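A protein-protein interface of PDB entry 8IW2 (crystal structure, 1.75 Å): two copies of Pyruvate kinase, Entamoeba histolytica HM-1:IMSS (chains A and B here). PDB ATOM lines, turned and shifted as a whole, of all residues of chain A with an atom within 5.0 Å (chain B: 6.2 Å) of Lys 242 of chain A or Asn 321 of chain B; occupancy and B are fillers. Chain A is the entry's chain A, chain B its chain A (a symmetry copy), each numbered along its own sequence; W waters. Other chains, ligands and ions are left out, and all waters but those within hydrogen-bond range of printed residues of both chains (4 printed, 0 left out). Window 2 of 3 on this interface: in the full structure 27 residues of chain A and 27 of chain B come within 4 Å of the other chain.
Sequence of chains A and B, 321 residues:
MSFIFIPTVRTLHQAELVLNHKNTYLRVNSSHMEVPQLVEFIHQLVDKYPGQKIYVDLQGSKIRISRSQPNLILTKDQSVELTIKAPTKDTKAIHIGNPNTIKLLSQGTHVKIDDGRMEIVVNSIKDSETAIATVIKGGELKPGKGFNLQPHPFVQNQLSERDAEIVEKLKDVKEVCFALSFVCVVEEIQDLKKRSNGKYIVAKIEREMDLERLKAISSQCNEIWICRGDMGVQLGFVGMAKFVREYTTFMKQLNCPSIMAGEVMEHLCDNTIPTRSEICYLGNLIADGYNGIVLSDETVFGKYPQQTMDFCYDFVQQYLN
NZ of Lys 242 of chain A sits at hydrogen-bond distance from O of Asn 321 of chain B, at 3.4 Å. The backbone carbonyl oxygen (O) of Tyr 319 of chain B sits at hydrogen-bond distance from the side-chain amino group (NZ) of Lys 242 of chain A (2.8 Å).
Among the printed residues, merely in contact across the chains: Val 238 of chain A with Gln 318 of chain B (3.7 Å), Val 238 of chain A with Tyr 319 of chain B (3.9 Å), Arg 245 of chain A with Asn 284 of chain B (3.8 Å) and Arg 245 of chain A with Tyr 319 of chain B (3.95 Å).
Of the printed residues of chain B, Val 238 of chain A touches Gln 318 and Tyr 319. Lys 242 of chain A touches two residues of chain B. Val 244 of chain A touches none of the printed residues of chain B. Of the printed residues of chain B, Arg 245 of chain A touches Asn 284 and Tyr 319. Of the printed residues of chain A, Asn 284 of chain B touches Arg 245 (3.8 Å). Of the printed residues of chain A, Gln 318 of chain B touches Val 238 (3.7 Å). Printed residues of chain A within 4 Å of Tyr 319 of chain B: Val 238 (3.9 Å), Lys 242 (2.8 Å) and Arg 245 (3.95 Å). Of chain A, only Lys 242 (3.4 Å) comes within 4 Å of Asn 321 of chain B. The nearest printed residue of chain A that does not touch Asn 321 of chain B is Val 238 of chain A (6.7 Å). The nearest printed residue of chain A that does not touch Asn 284 of chain B is Ala 241 of chain A (4.4 Å).
Printed residues of chain B that touch a printed residue of chain A: Asn 284, Gln 318, Tyr 319 and Asn 321. Hydrophobic or aromatic side chains of chain B within 4 Å of the printed part of chain A: Tyr 319. Hydrophobic or aromatic side chains of chain A that line the printed part of chain B: Val 238. Along chain A the printed residues that touch a printed residue of chain B span positions 238 to 245. Among the printed residues, no Asp or Glu carboxylate lies within 4 Å of a Lys or Arg side-chain nitrogen of the other chain.
No position is printed for both chains. Of the 6 pairs that touch across the chains among the printed residues, none has its exchanged pair printed and touching as well.
Water W2 lies within hydrogen-bond range of OH of Tyr 319 of chain B, OD1 of Asn 284 of chain B and O of Ala 241 of chain A. Water W1 lies within hydrogen-bond range of the backbone carbonyl oxygen of Ala 241 of chain A (2.7 Å) and the side-chain amide oxygen of Asn 284 of chain B (2.9 Å). Water W3 bridges the backbone NH of Gly 239 of chain A (2.8 Å) and the side-chain amide nitrogen of Gln 318 of chain B (3.5 Å). Water W4 bridges the side-chain amide oxygen of Gln 318 of chain B (2.9 Å) and the backbone NH of Val 238 of chain A (3.0 Å).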
ATOM      1  N   VAL A 238       2.451   7.361 -28.757  1.00  0.00           N
ATOM      2  CA  VAL A 238       3.517   6.546 -29.297  1.00  0.00           C
ATOM      3  C   VAL A 238       4.796   7.354 -29.471  1.00  0.00           C
ATOM      4  O   VAL A 238       5.914   6.920 -29.098  1.00  0.00           O
ATOM      5  CB  VAL A 238       3.074   5.878 -30.619  1.00  0.00           C
ATOM      6  CG1 VAL A 238       4.279   5.284 -31.349  1.00  0.00           C
ATOM      7  CG2 VAL A 238       2.056   4.818 -30.302  1.00  0.00           C
ATOM      8  N   GLY A 239       4.648   8.546 -30.083  1.00  0.00           N
ATOM      9  CA  GLY A 239       5.826   9.401 -30.266  1.00  0.00           C
ATOM     10  C   GLY A 239       6.498   9.791 -28.934  1.00  0.00           C
ATOM     11  O   GLY A 239       7.739   9.729 -28.842  1.00  0.00           O
ATOM     12  N   MET A 240       5.696  10.038 -27.880  1.00  0.00           N
ATOM     13  CA  MET A 240       6.266  10.294 -26.556  1.00  0.00           C
ATOM     14  C   MET A 240       7.034   9.086 -26.086  1.00  0.00           C
ATOM     15  O   MET A 240       8.135   9.265 -25.565  1.00  0.00           O
ATOM     16  CB  MET A 240       5.256  10.601 -25.426  1.00  0.00           C
ATOM     17  CG  MET A 240       5.771  10.259 -23.866  1.00  0.00           C
ATOM     18  SD  MET A 240       4.204  10.771 -22.920  1.00  0.00           S
ATOM     19  CE  MET A 240       3.470   9.028 -23.259  1.00  0.00           C
ATOM     20  N   ALA A 241       6.421   7.867 -26.144  1.00  0.00           N
ATOM     21  CA  ALA A 241       7.028   6.679 -25.576  1.00  0.00           C
ATOM     22  C   ALA A 241       8.355   6.420 -26.276  1.00  0.00           C
ATOM     23  O   ALA A 241       9.340   6.084 -25.654  1.00  0.00           O
ATOM     24  CB  ALA A 241       6.104   5.503 -25.715  1.00  0.00           C
ATOM     25  N   LYS A 242       8.348   6.546 -27.570  1.00  0.00           N
ATOM     26  CA  LYS A 242       9.556   6.340 -28.352  1.00  0.00           C
ATOM     27  C   LYS A 242      10.649   7.337 -27.973  1.00  0.00           C
ATOM     28  O   LYS A 242      11.795   6.953 -27.853  1.00  0.00           O
ATOM     29  CB  LYS A 242       9.156   6.372 -29.820  1.00  0.00           C
ATOM     30  CG  LYS A 242       8.644   5.030 -30.315  1.00  0.00           C
ATOM     31  CD  LYS A 242       8.192   4.985 -31.717  1.00  0.00           C
ATOM     32  CE  LYS A 242       8.109   3.572 -32.258  1.00  0.00           C
ATOM     33  NZ  LYS A 242       7.665   3.597 -33.664  1.00  0.00           N
ATOM     34  N   PHE A 243      10.334   8.628 -27.969  1.00  0.00           N
ATOM     35  CA  PHE A 243      11.322   9.643 -27.667  1.00  0.00           C
ATOM     36  C   PHE A 243      11.859   9.534 -26.248  1.00  0.00           C
ATOM     37  O   PHE A 243      13.056   9.593 -26.059  1.00  0.00           O
ATOM     38  CB  PHE A 243      10.832  11.064 -27.958  1.00  0.00           C
ATOM     39  CG  PHE A 243      11.875  12.091 -27.599  1.00  0.00           C
ATOM     40  CD1 PHE A 243      13.061  12.153 -28.335  1.00  0.00           C
ATOM     41  CD2 PHE A 243      11.735  12.905 -26.492  1.00  0.00           C
ATOM     42  CE1 PHE A 243      14.041  13.065 -28.007  1.00  0.00           C
ATOM     43  CE2 PHE A 243      12.751  13.799 -26.140  1.00  0.00           C
ATOM     44  CZ  PHE A 243      13.888  13.872 -26.918  1.00  0.00           C
ATOM     45  N   VAL A 244      11.036   9.311 -25.198  1.00  0.00           N
ATOM     46  CA  VAL A 244      11.621   9.173 -23.870  1.00  0.00           C
ATOM     47  C   VAL A 244      12.617   8.015 -23.840  1.00  0.00           C
ATOM     48  O   VAL A 244      13.621   8.098 -23.171  1.00  0.00           O
ATOM     49  CB  VAL A 244      10.528   8.949 -22.804  1.00  0.00           C
ATOM     50  CG1 VAL A 244      11.190   8.817 -21.430  1.00  0.00           C
ATOM     51  CG2 VAL A 244       9.591  10.110 -22.783  1.00  0.00           C
ATOM     52  N   ARG A 245      12.300   6.888 -24.487  1.00  0.00           N
ATOM     53  CA  ARG A 245      13.234   5.777 -24.559  1.00  0.00           C
ATOM     54  C   ARG A 245      14.535   6.155 -25.300  1.00  0.00           C
ATOM     55  O   ARG A 245      15.613   5.793 -24.859  1.00  0.00           O
ATOM     56  CB  ARG A 245      12.595   4.587 -25.298  1.00  0.00           C
ATOM     57  CG  ARG A 245      13.423   3.321 -25.205  1.00  0.00           C
ATOM     58  CD  ARG A 245      12.815   2.219 -26.066  1.00  0.00           C
ATOM     59  NE  ARG A 245      13.684   1.042 -26.116  1.00  0.00           N
ATOM     60  CZ  ARG A 245      13.783   0.143 -25.151  1.00  0.00           C
ATOM     61  NH1 ARG A 245      13.123   0.292 -24.014  1.00  0.00           N
ATOM     62  NH2 ARG A 245      14.518  -0.943 -25.365  1.00  0.00           N
ATOM     63  N   GLU A 246      14.413   6.887 -26.392  1.00  0.00           N
ATOM     64  CA  GLU A 246      15.596   7.280 -27.154  1.00  0.00           C
ATOM     65  C   GLU A 246      16.455   8.210 -26.293  1.00  0.00           C
ATOM     66  O   GLU A 246      17.675   8.003 -26.158  1.00  0.00           O
ATOM     67  CB  GLU A 246      15.190   7.938 -28.474  1.00  0.00           C
ATOM     68  CG  GLU A 246      16.385   8.190 -29.348  1.00  0.00           C
ATOM     69  CD  GLU A 246      16.145   9.026 -30.600  1.00  0.00           C
ATOM     70  OE1 GLU A 246      14.968   9.372 -30.885  1.00  0.00           O
ATOM     71  OE2 GLU A 246      17.162   9.341 -31.281  1.00  0.00           O
ATOM     72  N   ASN B 284       8.067   0.511 -23.806  1.00  0.00           N
ATOM     73  CA  ASN B 284       9.338  -0.082 -23.455  1.00  0.00           C
ATOM     74  C   ASN B 284       9.260  -1.590 -23.448  1.00  0.00           C
ATOM     75  O   ASN B 284      10.234  -2.288 -23.810  1.00  0.00           O
ATOM     76  CB  ASN B 284       9.856   0.461 -22.133  1.00  0.00           C
ATOM     77  CG  ASN B 284      10.165   1.959 -22.158  1.00  0.00           C
ATOM     78  OD1 ASN B 284      10.128   2.571 -23.206  1.00  0.00           O
ATOM     79  ND2 ASN B 284      10.425   2.528 -21.011  1.00  0.00           N
ATOM     80  N   VAL B 316       0.103  -0.561 -29.838  1.00  0.00           N
ATOM     81  CA  VAL B 316       1.135  -1.482 -30.306  1.00  0.00           C
ATOM     82  C   VAL B 316       1.302  -1.407 -31.807  1.00  0.00           C
ATOM     83  O   VAL B 316       2.444  -1.370 -32.285  1.00  0.00           O
ATOM     84  CB  VAL B 316       0.804  -2.920 -29.826  1.00  0.00           C
ATOM     85  CG1 VAL B 316       1.697  -3.967 -30.475  1.00  0.00           C
ATOM     86  CG2 VAL B 316       0.818  -2.954 -28.291  1.00  0.00           C
ATOM     87  N   GLN B 317       0.187  -1.418 -32.561  1.00  0.00           N
ATOM     88  CA  GLN B 317       0.296  -1.384 -33.999  1.00  0.00           C
ATOM     89  C   GLN B 317       1.133  -0.184 -34.433  1.00  0.00           C
ATOM     90  O   GLN B 317       2.073  -0.317 -35.208  1.00  0.00           O
ATOM     91  CB  GLN B 317      -1.131  -1.497 -34.532  1.00  0.00           C
ATOM     92  CG  GLN B 317      -1.490  -0.614 -35.694  1.00  0.00           C
ATOM     93  CD  GLN B 317      -2.803  -0.978 -36.328  1.00  0.00           C
ATOM     94  OE1 GLN B 317      -2.826  -1.836 -37.149  1.00  0.00           O
ATOM     95  NE2 GLN B 317      -3.902  -0.461 -35.825  1.00  0.00           N
ATOM     96  N   GLN B 318       0.727   1.016 -34.006  1.00  0.00           N
ATOM     97  CA  GLN B 318       1.451   2.255 -34.298  1.00  0.00           C
ATOM     98  C   GLN B 318       2.901   2.216 -33.806  1.00  0.00           C
ATOM     99  O   GLN B 318       3.799   2.686 -34.514  1.00  0.00           O
ATOM    100  CB  GLN B 318       0.746   3.456 -33.672  1.00  0.00           C
ATOM    101  CG  GLN B 318       1.355   4.783 -34.192  1.00  0.00           C
ATOM    102  CD  GLN B 318       0.649   6.019 -33.663  1.00  0.00           C
ATOM    103  OE1 GLN B 318      -0.310   5.965 -32.903  1.00  0.00           O
ATOM    104  NE2 GLN B 318       1.199   7.177 -33.979  1.00  0.00           N
ATOM    105  N   TYR B 319       3.134   1.688 -32.604  1.00  0.00           N
ATOM    106  CA  TYR B 319       4.493   1.516 -32.131  1.00  0.00           C
ATOM    107  C   TYR B 319       5.347   0.726 -33.091  1.00  0.00           C
ATOM    108  O   TYR B 319       6.489   1.105 -33.343  1.00  0.00           O
ATOM    109  CB  TYR B 319       4.516   0.936 -30.716  1.00  0.00           C
ATOM    110  CG  TYR B 319       5.825   1.157 -29.985  1.00  0.00           C
ATOM    111  CD1 TYR B 319       6.921   0.331 -30.201  1.00  0.00           C
ATOM    112  CD2 TYR B 319       5.965   2.191 -29.078  1.00  0.00           C
ATOM    113  CE1 TYR B 319       8.102   0.526 -29.517  1.00  0.00           C
ATOM    114  CE2 TYR B 319       7.131   2.392 -28.367  1.00  0.00           C
ATOM    115  CZ  TYR B 319       8.237   1.596 -28.667  1.00  0.00           C
ATOM    116  OH  TYR B 319       9.388   1.814 -27.998  1.00  0.00           O
ATOM    117  N   LEU B 320       4.858  -0.412 -33.576  1.00  0.00           N
ATOM    118  CA  LEU B 320       5.654  -1.279 -34.440  1.00  0.00           C
ATOM    119  C   LEU B 320       5.918  -0.625 -35.815  1.00  0.00           C
ATOM    120  O   LEU B 320       6.794  -1.075 -36.523  1.00  0.00           O
ATOM    121  CB  LEU B 320       4.922  -2.612 -34.625  1.00  0.00           C
ATOM    122  CG  LEU B 320       4.719  -3.410 -33.343  1.00  0.00           C
ATOM    123  CD1 LEU B 320       3.870  -4.636 -33.612  1.00  0.00           C
ATOM    124  CD2 LEU B 320       6.042  -3.799 -32.728  1.00  0.00           C
ATOM    125  N   ASN B 321       5.136   0.364 -36.262  1.00  0.00           N
ATOM    126  CA  ASN B 321       5.392   1.022 -37.536  1.00  0.00           C
ATOM    127  C   ASN B 321       5.848   2.464 -37.307  1.00  0.00           C
ATOM    128  O   ASN B 321       7.011   2.603 -36.820  1.00  0.00           O
ATOM    129  CB  ASN B 321       4.157   1.077 -38.427  1.00  0.00           C
ATOM    130  CG  ASN B 321       3.471  -0.251 -38.689  1.00  0.00           C
ATOM    131  OD1 ASN B 321       4.072  -1.307 -38.906  1.00  0.00           O
ATOM    132  ND2 ASN B 321       2.151  -0.199 -38.735  1.00  0.00           N
HETATM  133  O   HOH W   1       9.215   5.290 -23.047  1.00  0.00           O
HETATM  134  O   HOH W   2       9.170   3.116 -25.727  1.00  0.00           O
HETATM  135  O   HOH W   3       2.507   9.453 -31.665  1.00  0.00           O
HETATM  136  O   HOH W   4       0.007   7.547 -30.489  1.00  0.00           O
